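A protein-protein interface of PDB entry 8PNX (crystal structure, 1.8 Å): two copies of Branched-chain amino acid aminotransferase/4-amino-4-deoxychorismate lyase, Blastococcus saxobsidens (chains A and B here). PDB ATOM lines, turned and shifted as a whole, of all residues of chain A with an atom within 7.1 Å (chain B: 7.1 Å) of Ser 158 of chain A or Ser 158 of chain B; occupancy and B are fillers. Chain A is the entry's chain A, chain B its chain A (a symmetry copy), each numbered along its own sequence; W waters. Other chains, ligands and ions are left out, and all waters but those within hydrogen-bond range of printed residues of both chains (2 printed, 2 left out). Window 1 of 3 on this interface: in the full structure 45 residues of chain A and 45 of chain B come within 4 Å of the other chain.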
ATOM      1  N   GLY A  31      -4.541  18.818 -12.861  1.00  0.00           N
ATOM      2  CA  GLY A  31      -3.599  19.773 -12.249  1.00  0.00           C
ATOM      3  C   GLY A  31      -2.734  19.032 -11.254  1.00  0.00           C
ATOM      4  O   GLY A  31      -1.540  19.290 -11.188  1.00  0.00           O
ATOM      5  N   LEU A  32      -3.318  18.088 -10.525  1.00  0.00           N
ATOM      6  CA  LEU A  32      -2.541  17.250  -9.593  1.00  0.00           C
ATOM      7  C   LEU A  32      -1.761  16.159 -10.342  1.00  0.00           C
ATOM      8  O   LEU A  32      -0.533  16.034 -10.096  1.00  0.00           O
ATOM      9  CB  LEU A  32      -3.499  16.641  -8.587  1.00  0.00           C
ATOM     10  CG  LEU A  32      -2.916  15.543  -7.715  1.00  0.00           C
ATOM     11  CD1 LEU A  32      -1.836  16.122  -6.869  1.00  0.00           C
ATOM     12  CD2 LEU A  32      -4.025  14.913  -6.865  1.00  0.00           C
ATOM     13  N   GLY A  33      -2.427  15.349 -11.170  1.00  0.00           N
ATOM     14  CA  GLY A  33      -1.792  14.117 -11.699  1.00  0.00           C
ATOM     15  C   GLY A  33      -0.832  14.372 -12.833  1.00  0.00           C
ATOM     16  O   GLY A  33       0.097  13.519 -13.050  1.00  0.00           O
ATOM     17  N   ARG A  34      -1.006  15.479 -13.549  1.00  0.00           N
ATOM     18  CA  ARG A  34      -0.162  15.838 -14.715  1.00  0.00           C
ATOM     19  C   ARG A  34       0.496  17.227 -14.571  1.00  0.00           C
ATOM     20  O   ARG A  34       1.205  17.626 -15.501  1.00  0.00           O
ATOM     21  CB  ARG A  34      -1.018  15.763 -15.984  1.00  0.00           C
ATOM     22  CG  ARG A  34      -1.434  14.344 -16.340  1.00  0.00           C
ATOM     23  CD  ARG A  34      -0.257  13.463 -16.769  1.00  0.00           C
ATOM     24  NE  ARG A  34      -0.728  12.111 -17.129  1.00  0.00           N
ATOM     25  CZ  ARG A  34       0.040  11.041 -17.384  1.00  0.00           C
ATOM     26  NH1 ARG A  34       1.351  11.102 -17.288  1.00  0.00           N
ATOM     27  NH2 ARG A  34      -0.529   9.898 -17.716  1.00  0.00           N
ATOM     28  N   GLY A  35       0.210  18.001 -13.512  1.00  0.00           N
ATOM     29  CA  GLY A  35       0.772  19.352 -13.401  1.00  0.00           C
ATOM     30  C   GLY A  35       0.287  20.191 -14.550  1.00  0.00           C
ATOM     31  O   GLY A  35       1.001  21.130 -14.938  1.00  0.00           O
ATOM     32  N   ASP A  36      -0.912  19.855 -15.052  1.00  0.00           N
ATOM     33  CA  ASP A  36      -1.527  20.377 -16.297  1.00  0.00           C
ATOM     34  C   ASP A  36      -2.527  21.468 -15.920  1.00  0.00           C
ATOM     35  O   ASP A  36      -3.767  21.255 -15.811  1.00  0.00           O
ATOM     36  CB  ASP A  36      -2.110  19.250 -17.135  1.00  0.00           C
ATOM     37  CG  ASP A  36      -2.486  19.670 -18.531  1.00  0.00           C
ATOM     38  OD1 ASP A  36      -2.104  20.820 -18.949  1.00  0.00           O
ATOM     39  OD2 ASP A  36      -3.178  18.849 -19.182  1.00  0.00           O
ATOM     40  N   GLY A  37      -1.981  22.670 -15.778  1.00  0.00           N
ATOM     41  CA  GLY A  37      -2.773  23.844 -15.409  1.00  0.00           C
ATOM     42  C   GLY A  37      -1.855  25.035 -15.423  1.00  0.00           C
ATOM     43  O   GLY A  37      -0.611  24.883 -15.761  1.00  0.00           O
ATOM     44  N   ILE A  38      -2.427  26.184 -15.097  1.00  0.00           N
ATOM     45  CA  ILE A  38      -1.603  27.413 -15.033  1.00  0.00           C
ATOM     46  C   ILE A  38      -1.854  28.088 -13.705  1.00  0.00           C
ATOM     47  O   ILE A  38      -2.818  27.751 -13.046  1.00  0.00           O
ATOM     48  CB  ILE A  38      -1.827  28.322 -16.245  1.00  0.00           C
ATOM     49  CG1 ILE A  38      -3.268  28.792 -16.429  1.00  0.00           C
ATOM     50  CG2 ILE A  38      -1.312  27.586 -17.469  1.00  0.00           C
ATOM     51  CD1 ILE A  38      -3.738  29.911 -15.517  1.00  0.00           C
ATOM     52  N   PHE A  39      -0.986  29.022 -13.354  1.00  0.00           N
ATOM     53  CA  PHE A  39      -1.272  29.829 -12.161  1.00  0.00           C
ATOM     54  C   PHE A  39      -0.644  31.208 -12.261  1.00  0.00           C
ATOM     55  O   PHE A  39       0.089  31.548 -13.208  1.00  0.00           O
ATOM     56  CB  PHE A  39      -0.795  29.124 -10.904  1.00  0.00           C
ATOM     57  CG  PHE A  39       0.668  29.260 -10.643  1.00  0.00           C
ATOM     58  CD1 PHE A  39       1.573  28.515 -11.369  1.00  0.00           C
ATOM     59  CD2 PHE A  39       1.128  30.124  -9.665  1.00  0.00           C
ATOM     60  CE1 PHE A  39       2.922  28.586 -11.101  1.00  0.00           C
ATOM     61  CE2 PHE A  39       2.484  30.185  -9.392  1.00  0.00           C
ATOM     62  CZ  PHE A  39       3.370  29.422 -10.114  1.00  0.00           C
ATOM     63  N   LEU A 151       6.260  24.975 -23.845  1.00  0.00           N
ATOM     64  CA  LEU A 151       5.448  25.890 -22.998  1.00  0.00           C
ATOM     65  C   LEU A 151       6.299  27.057 -22.450  1.00  0.00           C
ATOM     66  O   LEU A 151       5.933  27.612 -21.388  1.00  0.00           O
ATOM     67  CB  LEU A 151       4.781  25.099 -21.874  1.00  0.00           C
ATOM     68  CG  LEU A 151       3.804  24.018 -22.339  1.00  0.00           C
ATOM     69  CD1 LEU A 151       3.128  23.347 -21.140  1.00  0.00           C
ATOM     70  CD2 LEU A 151       2.780  24.597 -23.305  1.00  0.00           C
ATOM     71  N   LYS A 155       3.130  30.074 -17.510  1.00  0.00           N
ATOM     72  CA  LYS A 155       3.345  29.889 -16.062  1.00  0.00           C
ATOM     73  C   LYS A 155       2.441  28.734 -15.616  1.00  0.00           C
ATOM     74  O   LYS A 155       1.261  28.988 -15.429  1.00  0.00           O
ATOM     75  CB  LYS A 155       2.997  31.198 -15.350  1.00  0.00           C
ATOM     76  CG  LYS A 155       3.448  31.264 -13.913  1.00  0.00           C
ATOM     77  CD  LYS A 155       3.301  32.657 -13.298  1.00  0.00           C
ATOM     78  CE  LYS A 155       3.240  32.536 -11.796  1.00  0.00           C
ATOM     79  NZ  LYS A 155       4.461  31.831 -11.340  1.00  0.00           N
ATOM     80  N   THR A 156       2.964  27.513 -15.648  1.00  0.00           N
ATOM     81  CA  THR A 156       2.234  26.233 -15.504  1.00  0.00           C
ATOM     82  C   THR A 156       2.323  25.764 -14.057  1.00  0.00           C
ATOM     83  O   THR A 156       3.170  26.275 -13.297  1.00  0.00           O
ATOM     84  CB  THR A 156       2.773  25.168 -16.473  1.00  0.00           C
ATOM     85  OG1 THR A 156       3.985  24.650 -15.938  1.00  0.00           O
ATOM     86  CG2 THR A 156       2.993  25.697 -17.876  1.00  0.00           C
ATOM     87  N   LEU A 157       1.539  24.753 -13.705  1.00  0.00           N
ATOM     88  CA  LEU A 157       1.684  24.046 -12.418  1.00  0.00           C
ATOM     89  C   LEU A 157       2.873  23.070 -12.394  1.00  0.00           C
ATOM     90  O   LEU A 157       3.153  22.512 -11.301  1.00  0.00           O
ATOM     91  CB  LEU A 157       0.339  23.381 -12.117  1.00  0.00           C
ATOM     92  CG  LEU A 157      -0.795  24.372 -11.893  1.00  0.00           C
ATOM     93  CD1 LEU A 157      -2.102  23.650 -11.833  1.00  0.00           C
ATOM     94  CD2 LEU A 157      -0.591  25.175 -10.628  1.00  0.00           C
ATOM     95  N   SER A 158       3.590  22.886 -13.499  1.00  0.00           N
ATOM     96  CA  SER A 158       4.637  21.841 -13.650  1.00  0.00           C
ATOM     97  C   SER A 158       5.993  22.405 -13.236  1.00  0.00           C
ATOM     98  O   SER A 158       6.864  22.636 -14.145  1.00  0.00           O
ATOM     99  CB  SER A 158       4.674  21.263 -15.017  1.00  0.00           C
ATOM    100  OG  SER A 158       3.609  20.346 -15.147  1.00  0.00           O
ATOM    101  N   TYR A 159       6.134  22.743 -11.953  1.00  0.00           N
ATOM    102  CA  TYR A 159       7.375  23.429 -11.477  1.00  0.00           C
ATOM    103  C   TYR A 159       8.278  22.449 -10.738  1.00  0.00           C
ATOM    104  O   TYR A 159       9.062  22.904  -9.889  1.00  0.00           O
ATOM    105  CB  TYR A 159       7.061  24.601 -10.545  1.00  0.00           C
ATOM    106  CG  TYR A 159       7.005  25.967 -11.194  1.00  0.00           C
ATOM    107  CD1 TYR A 159       6.167  26.208 -12.261  1.00  0.00           C
ATOM    108  CD2 TYR A 159       7.689  27.061 -10.672  1.00  0.00           C
ATOM    109  CE1 TYR A 159       6.026  27.476 -12.817  1.00  0.00           C
ATOM    110  CE2 TYR A 159       7.577  28.336 -11.231  1.00  0.00           C
ATOM    111  CZ  TYR A 159       6.709  28.558 -12.289  1.00  0.00           C
ATOM    112  OH  TYR A 159       6.574  29.767 -12.938  1.00  0.00           O
ATOM    113  N   ALA A 160       8.221  21.145 -11.018  1.00  0.00           N
ATOM    114  CA  ALA A 160       9.076  20.204 -10.244  1.00  0.00           C
ATOM    115  C   ALA A 160      10.562  20.558 -10.409  1.00  0.00           C
ATOM    116  O   ALA A 160      11.326  20.553  -9.393  1.00  0.00           O
ATOM    117  CB  ALA A 160       8.771  18.773 -10.633  1.00  0.00           C
ATOM    118  N   VAL A 161      10.995  20.798 -11.638  1.00  0.00           N
ATOM    119  CA  VAL A 161      12.385  21.165 -11.994  1.00  0.00           C
ATOM    120  C   VAL A 161      12.780  22.476 -11.302  1.00  0.00           C
ATOM    121  O   VAL A 161      13.898  22.520 -10.732  1.00  0.00           O
ATOM    122  CB  VAL A 161      12.515  21.282 -13.525  1.00  0.00           C
ATOM    123  CG1 VAL A 161      13.809  21.942 -13.887  1.00  0.00           C
ATOM    124  CG2 VAL A 161      12.361  19.919 -14.174  1.00  0.00           C
ATOM    125  N   ASN A 162      11.903  23.466 -11.367  1.00  0.00           N
ATOM    126  CA  ASN A 162      12.038  24.807 -10.715  1.00  0.00           C
ATOM    127  C   ASN A 162      12.327  24.597  -9.233  1.00  0.00           C
ATOM    128  O   ASN A 162      13.309  25.140  -8.748  1.00  0.00           O
ATOM    129  CB  ASN A 162      10.779  25.653 -10.871  1.00  0.00           C
ATOM    130  CG  ASN A 162      10.385  25.829 -12.320  1.00  0.00           C
ATOM    131  OD1 ASN A 162      10.109  24.829 -13.007  1.00  0.00           O
ATOM    132  ND2 ASN A 162      10.381  27.072 -12.780  1.00  0.00           N
ATOM    133  N   GLY B  31       1.925  19.110  -4.647  1.00  0.00           N
ATOM    134  CA  GLY B  31       1.700  18.256  -5.827  1.00  0.00           C
ATOM    135  C   GLY B  31       0.802  18.992  -6.797  1.00  0.00           C
ATOM    136  O   GLY B  31       1.039  18.934  -7.996  1.00  0.00           O
ATOM    137  N   LEU B  32      -0.185  19.716  -6.282  1.00  0.00           N
ATOM    138  CA  LEU B  32      -1.057  20.541  -7.138  1.00  0.00           C
ATOM    139  C   LEU B  32      -0.355  21.840  -7.563  1.00  0.00           C
ATOM    140  O   LEU B  32      -0.350  22.137  -8.786  1.00  0.00           O
ATOM    141  CB  LEU B  32      -2.333  20.837  -6.374  1.00  0.00           C
ATOM    142  CG  LEU B  32      -3.234  21.891  -6.995  1.00  0.00           C
ATOM    143  CD1 LEU B  32      -3.717  21.395  -8.313  1.00  0.00           C
ATOM    144  CD2 LEU B  32      -4.396  22.202  -6.046  1.00  0.00           C
ATOM    145  N   GLY B  33       0.161  22.628  -6.617  1.00  0.00           N
ATOM    146  CA  GLY B  33       0.597  24.010  -6.936  1.00  0.00           C
ATOM    147  C   GLY B  33       1.937  24.077  -7.623  1.00  0.00           C
ATOM    148  O   GLY B  33       2.200  25.097  -8.350  1.00  0.00           O
ATOM    149  N   ARG B  34       2.776  23.063  -7.434  1.00  0.00           N
ATOM    150  CA  ARG B  34       4.140  23.013  -8.016  1.00  0.00           C
ATOM    151  C   ARG B  34       4.378  21.750  -8.871  1.00  0.00           C
ATOM    152  O   ARG B  34       5.492  21.605  -9.385  1.00  0.00           O
ATOM    153  CB  ARG B  34       5.164  23.112  -6.881  1.00  0.00           C
ATOM    154  CG  ARG B  34       5.176  24.474  -6.206  1.00  0.00           C
ATOM    155  CD  ARG B  34       5.691  25.592  -7.117  1.00  0.00           C
ATOM    156  NE  ARG B  34       5.706  26.881  -6.396  1.00  0.00           N
ATOM    157  CZ  ARG B  34       5.935  28.089  -6.930  1.00  0.00           C
ATOM    158  NH1 ARG B  34       6.134  28.240  -8.222  1.00  0.00           N
ATOM    159  NH2 ARG B  34       5.938  29.153  -6.150  1.00  0.00           N
ATOM    160  N   GLY B  35       3.430  20.803  -8.952  1.00  0.00           N
ATOM    161  CA  GLY B  35       3.673  19.565  -9.701  1.00  0.00           C
ATOM    162  C   GLY B  35       4.817  18.818  -9.074  1.00  0.00           C
ATOM    163  O   GLY B  35       5.503  18.074  -9.795  1.00  0.00           O
ATOM    164  N   ASP B  36       4.986  19.010  -7.756  1.00  0.00           N
ATOM    165  CA  ASP B  36       6.140  18.563  -6.938  1.00  0.00           C
ATOM    166  C   ASP B  36       5.749  17.277  -6.213  1.00  0.00           C
ATOM    167  O   ASP B  36       5.342  17.260  -5.017  1.00  0.00           O
ATOM    168  CB  ASP B  36       6.629  19.677  -6.027  1.00  0.00           C
ATOM    169  CG  ASP B  36       7.963  19.391  -5.389  1.00  0.00           C
ATOM    170  OD1 ASP B  36       8.643  18.389  -5.812  1.00  0.00           O
ATOM    171  OD2 ASP B  36       8.301  20.162  -4.458  1.00  0.00           O
ATOM    172  N   GLY B  37       5.933  16.177  -6.934  1.00  0.00           N
ATOM    173  CA  GLY B  37       5.608  14.847  -6.418  1.00  0.00           C
ATOM    174  C   GLY B  37       6.021  13.842  -7.458  1.00  0.00           C
ATOM    175  O   GLY B  37       6.587  14.248  -8.553  1.00  0.00           O
ATOM    176  N   ILE B  38       5.779  12.580  -7.140  1.00  0.00           N
ATOM    177  CA  ILE B  38       6.104  11.511  -8.113  1.00  0.00           C
ATOM    178  C   ILE B  38       4.887  10.631  -8.279  1.00  0.00           C
ATOM    179  O   ILE B  38       3.989  10.708  -7.463  1.00  0.00           O
ATOM    180  CB  ILE B  38       7.376  10.749  -7.732  1.00  0.00           C
ATOM    181  CG1 ILE B  38       7.323  10.070  -6.365  1.00  0.00           C
ATOM    182  CG2 ILE B  38       8.539  11.719  -7.837  1.00  0.00           C
ATOM    183  CD1 ILE B  38       6.536   8.775  -6.280  1.00  0.00           C
ATOM    184  N   PHE B  39       4.895   9.819  -9.323  1.00  0.00           N
ATOM    185  CA  PHE B  39       3.823   8.822  -9.440  1.00  0.00           C
ATOM    186  C   PHE B  39       4.288   7.596 -10.206  1.00  0.00           C
ATOM    187  O   PHE B  39       5.413   7.516 -10.732  1.00  0.00           O
ATOM    188  CB  PHE B  39       2.596   9.422 -10.104  1.00  0.00           C
ATOM    189  CG  PHE B  39       2.682   9.503 -11.591  1.00  0.00           C
ATOM    190  CD1 PHE B  39       3.447  10.482 -12.188  1.00  0.00           C
ATOM    191  CD2 PHE B  39       1.987   8.606 -12.382  1.00  0.00           C
ATOM    192  CE1 PHE B  39       3.491  10.606 -13.560  1.00  0.00           C
ATOM    193  CE2 PHE B  39       2.025   8.741 -13.761  1.00  0.00           C
ATOM    194  CZ  PHE B  39       2.779   9.733 -14.338  1.00  0.00           C
ATOM    195  N   LEU B 151      15.851  16.414 -13.250  1.00  0.00           N
ATOM    196  CA  LEU B 151      15.017  15.268 -12.794  1.00  0.00           C
ATOM    197  C   LEU B 151      14.871  14.200 -13.900  1.00  0.00           C
ATOM    198  O   LEU B 151      13.865  13.453 -13.876  1.00  0.00           O
ATOM    199  CB  LEU B 151      13.658  15.776 -12.314  1.00  0.00           C
ATOM    200  CG  LEU B 151      13.713  16.728 -11.117  1.00  0.00           C
ATOM    201  CD1 LEU B 151      12.301  17.107 -10.662  1.00  0.00           C
ATOM    202  CD2 LEU B 151      14.521  16.118  -9.980  1.00  0.00           C
ATOM    203  N   LYS B 155       9.952  10.051 -12.434  1.00  0.00           N
ATOM    204  CA  LYS B 155       8.574  10.074 -12.961  1.00  0.00           C
ATOM    205  C   LYS B 155       7.755  10.988 -12.042  1.00  0.00           C
ATOM    206  O   LYS B 155       7.366  10.514 -10.985  1.00  0.00           O
ATOM    207  CB  LYS B 155       8.037   8.641 -12.971  1.00  0.00           C
ATOM    208  CG  LYS B 155       6.763   8.460 -13.756  1.00  0.00           C
ATOM    209  CD  LYS B 155       6.377   6.992 -13.950  1.00  0.00           C
ATOM    210  CE  LYS B 155       4.898   6.897 -14.232  1.00  0.00           C
ATOM    211  NZ  LYS B 155       4.602   7.732 -15.420  1.00  0.00           N
ATOM    212  N   THR B 156       7.691  12.273 -12.373  1.00  0.00           N
ATOM    213  CA  THR B 156       7.178  13.378 -11.533  1.00  0.00           C
ATOM    214  C   THR B 156       5.726  13.657 -11.899  1.00  0.00           C
ATOM    215  O   THR B 156       5.263  13.200 -12.964  1.00  0.00           O
ATOM    216  CB  THR B 156       8.045  14.640 -11.677  1.00  0.00           C
ATOM    217  OG1 THR B 156       7.702  15.280 -12.901  1.00  0.00           O
ATOM    218  CG2 THR B 156       9.531  14.350 -11.626  1.00  0.00           C
ATOM    219  N   LEU B 157       5.048  14.463 -11.093  1.00  0.00           N
ATOM    220  CA  LEU B 157       3.721  15.005 -11.444  1.00  0.00           C
ATOM    221  C   LEU B 157       3.787  16.157 -12.462  1.00  0.00           C
ATOM    222  O   LEU B 157       2.700  16.602 -12.917  1.00  0.00           O
ATOM    223  CB  LEU B 157       3.030  15.385 -10.132  1.00  0.00           C
ATOM    224  CG  LEU B 157       2.740  14.194  -9.229  1.00  0.00           C
ATOM    225  CD1 LEU B 157       2.279  14.670  -7.888  1.00  0.00           C
ATOM    226  CD2 LEU B 157       1.703  13.275  -9.834  1.00  0.00           C
ATOM    227  N   SER B 158       4.972  16.607 -12.864  1.00  0.00           N
ATOM    228  CA  SER B 158       5.164  17.825 -13.695  1.00  0.00           C
ATOM    229  C   SER B 158       5.152  17.449 -15.173  1.00  0.00           C
ATOM    230  O   SER B 158       6.252  17.494 -15.826  1.00  0.00           O
ATOM    231  CB  SER B 158       6.388  18.580 -13.327  1.00  0.00           C
ATOM    232  OG  SER B 158       6.130  19.311 -12.148  1.00  0.00           O
ATOM    233  N   TYR B 159       4.006  16.971 -15.659  1.00  0.00           N
ATOM    234  CA  TYR B 159       3.930  16.448 -17.059  1.00  0.00           C
ATOM    235  C   TYR B 159       3.247  17.458 -17.972  1.00  0.00           C
ATOM    236  O   TYR B 159       2.675  17.033 -18.989  1.00  0.00           O
ATOM    237  CB  TYR B 159       3.166  15.124 -17.136  1.00  0.00           C
ATOM    238  CG  TYR B 159       4.010  13.869 -17.112  1.00  0.00           C
ATOM    239  CD1 TYR B 159       4.898  13.635 -16.085  1.00  0.00           C
ATOM    240  CD2 TYR B 159       3.840  12.847 -18.042  1.00  0.00           C
ATOM    241  CE1 TYR B 159       5.618  12.447 -15.987  1.00  0.00           C
ATOM    242  CE2 TYR B 159       4.571  11.659 -17.972  1.00  0.00           C
ATOM    243  CZ  TYR B 159       5.440  11.437 -16.915  1.00  0.00           C
ATOM    244  OH  TYR B 159       6.241  10.321 -16.794  1.00  0.00           O
ATOM    245  N   ALA B 160       3.282  18.759 -17.675  1.00  0.00           N
ATOM    246  CA  ALA B 160       2.561  19.719 -18.555  1.00  0.00           C
ATOM    247  C   ALA B 160       3.098  19.648 -19.992  1.00  0.00           C
ATOM    248  O   ALA B 160       2.284  19.646 -20.969  1.00  0.00           O
ATOM    249  CB  ALA B 160       2.626  21.116 -17.976  1.00  0.00           C
ATOM    250  N   VAL B 161       4.414  19.652 -20.149  1.00  0.00           N
ATOM    251  CA  VAL B 161       5.117  19.578 -21.450  1.00  0.00           C
ATOM    252  C   VAL B 161       4.759  18.273 -22.172  1.00  0.00           C
ATOM    253  O   VAL B 161       4.457  18.343 -23.389  1.00  0.00           O
ATOM    254  CB  VAL B 161       6.637  19.693 -21.226  1.00  0.00           C
ATOM    255  CG1 VAL B 161       7.375  19.317 -22.474  1.00  0.00           C
ATOM    256  CG2 VAL B 161       6.996  21.084 -20.741  1.00  0.00           C
ATOM    257  N   ASN B 162       4.801  17.166 -21.445  1.00  0.00           N
ATOM    258  CA  ASN B 162       4.431  15.792 -21.912  1.00  0.00           C
ATOM    259  C   ASN B 162       3.032  15.847 -22.514  1.00  0.00           C
ATOM    260  O   ASN B 162       2.868  15.418 -23.647  1.00  0.00           O
ATOM    261  CB  ASN B 162       4.455  14.773 -20.778  1.00  0.00           C
ATOM    262  CG  ASN B 162       5.795  14.730 -20.077  1.00  0.00           C
ATOM    263  OD1 ASN B 162       6.226  15.751 -19.513  1.00  0.00           O
ATOM    264  ND2 ASN B 162       6.447  13.577 -20.131  1.00  0.00           N
HETATM  265  O   HOH W   1      -0.369  20.829 -20.838  1.00  0.00           O
HETATM  266  O   HOH W   2      10.833  18.930  -7.031  1.00  0.00           O
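Gly 31 of chain A touches Leu 32 of chain B, and with the chains exchanged Leu 32 of chain A touches Gly 31 of chain B. Leu 32 of chain A touches Leu 157 of chain B, and with the chains exchanged Leu 157 of chain A touches Leu 32 of chain B. Leu 151 of chain A touches Ala 160 of chain B, and with the chains exchanged Ala 160 of chain A touches Leu 151 of chain B. Ser 158 of chain A touches Ala 160 of chain B, and with the chains exchanged Ala 160 of chain A touches Ser 158 of chain B.
OG of Ser 158 of chain A lies within hydrogen-bond range of O of Gly 35 of chain A, 2.7 Å away. The backbone NH of Ser 158 of chain A is in hydrogen-bond range of the side-chain hydroxyl of Thr 156 of chain A. The backbone carbonyl oxygen (O) of Gly 37 of chain B lies within hydrogen-bond range of the backbone NH (N) of Leu 157 of chain B, at 3.0 Å. The backbone NH (N) of Phe 39 of chain B is in hydrogen-bond range of the backbone carbonyl oxygen (O) of Lys 155 of chain B (3.1 Å). The side-chain amino group of Lys 155 of chain B lies within hydrogen-bond range of the side-chain hydroxyl of Tyr 159 of chain B (3.4 Å). The side-chain hydroxyl of Thr 156 of chain B is in hydrogen-bond range of the backbone NH of Ser 158 of chain B (3.0 Å).
Hydrophobic or aromatic side chains of chain A that line the printed part of chain B: Leu 32, Phe 39, Leu 151, Leu 157, Tyr 159 and Ala 160. Of the 18 printed residues of chain B, 11 touch a printed residue of chain A. Hydrophobic or aromatic side chains of chain B within 4 Å of the printed part of chain A: Leu 32, Phe 39, Leu 151, Leu 157, Tyr 159 and Ala 160. Among the printed residues, 28 pairs touch across the chains. Among the printed residues, no Asp or Glu carboxylate lies within 4 Å of a Lys or Arg side-chain nitrogen of the other chain.
Printed residues of chain B within 4 Å of Gly 33 of chain A: Leu 157. Of the printed residues of chain B, Arg 34 of chain A touches Phe 39, Leu 157, Ser 158, Tyr 159 and Ala 160. Printed residues of chain B within 4 Å of Gly 35 of chain A: Leu 157 and Ala 160. Ile 38 of chain A touches none of the printed residues of chain B. Thr 156 of chain A touches none of the printed residues of chain B. Ser 158 of chain A touches just these residues of chain B: Arg 34, Ser 158, Tyr 159 and Ala 160. Of the printed residues of chain B, Tyr 159 of chain A touches Arg 34 and Ser 158. Of chain A, only Arg 34 (3.96 Å), Ser 158 (3.3 Å), Tyr 159 (3.4 Å) and Ala 160 (3.0 Å) come within 4 Å of Ser 158 of chain B. The nearest residue of chain B that does not touch Ser 158 of chain A is Leu 157 of chain B (4.5 Å). The nearest printed residue of chain B that does not touch Phe 39 of chain A is Gly 33 of chain B (4.5 Å).
Among the printed residues, merely in contact across the chains: Gly 31 of chain A with Leu 32 of chain B (3.9 Å), Leu 32 of chain A with Gly 31 of chain B (3.9 Å), Leu 32 of chain A with Leu 32 of chain B (3.998 Å), Leu 32 of chain A with Leu 157 of chain B (3.6 Å), Gly 33 of chain A with Leu 157 of chain B (3.6 Å), Arg 34 of chain A with Phe 39 of chain B (3.6 Å), Arg 34 of chain A with Ser 158 of chain B (3.96 Å), Gly 35 of chain A with Ala 160 of chain B (3.4 Å), Phe 39 of chain A with Arg 34 of chain B (3.6 Å), Leu 151 of chain A with Ala 160 of chain B (3.8 Å), Leu 157 of chain A with Leu 32 of chain B (3.6 Å), Leu 157 of chain A with Gly 33 of chain B (3.6 Å), Ser 158 of chain A with Arg 34 of chain B (3.96 Å), Ser 158 of chain A with Ser 158 of chain B (3.3 Å), Ala 160 of chain A with Gly 35 of chain B (3.4 Å) and Ala 160 of chain A with Leu 151 of chain B (3.8 Å).
Water W1 bridges OD1 of Asp 36 of chain A and O of Ala 160 of chain B. Water W2 bridges OD1 of Asp 36 of chain B and O of Ala 160 of chain A.
The backbone carbonyl oxygen of Arg 34 of chain A is in hydrogen-bond range of the backbone NH of Tyr 159 of chain B, 2.9 Å away. O of Arg 34 of chain A sits at hydrogen-bond distance from N of Ala 160 of chain B, at 3.2 Å. The backbone NH (N) of Gly 35 of chain A sits at hydrogen-bond distance from the backbone carbonyl oxygen (O) of Leu 157 of chain B (2.9 Å). The backbone NH (N) of Gly 35 of chain B lies within hydrogen-bond range of the backbone carbonyl oxygen (O) of Leu 157 of chain A (2.9 Å). The backbone NH (N) of Tyr 159 of chain B is in hydrogen-bond range of the side-chain hydroxyl (OG) of Ser 158 of chain A (3.4 Å). The backbone NH (N) of Ala 160 of chain B lies within hydrogen-bond range of the side-chain hydroxyl (OG) of Ser 158 of chain A (3.0 Å). The backbone NH (N) of Tyr 159 of chain A lies within hydrogen-bond range of the backbone carbonyl oxygen (O) of Arg 34 of chain B (2.9 Å). The backbone NH (N) of Tyr 159 of chain A sits at hydrogen-bond distance from the side-chain hydroxyl (OG) of Ser 158 of chain B, 3.4 Å away. The backbone carbonyl oxygen (O) of Arg 34 of chain B sits at hydrogen-bond distance from the backbone NH (N) of Ala 160 of chain A (3.2 Å). N of Ala 160 of chain A is in hydrogen-bond range of OG of Ser 158 of chain B. The backbone carbonyl oxygen of Arg 34 of chain A sits close to the backbone carbonyl oxygen of Leu 157 of chain B (3.2 Å). The backbone carbonyl oxygen of Leu 157 of chain A lies close to the backbone carbonyl oxygen of Arg 34 of chain B (3.2 Å).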
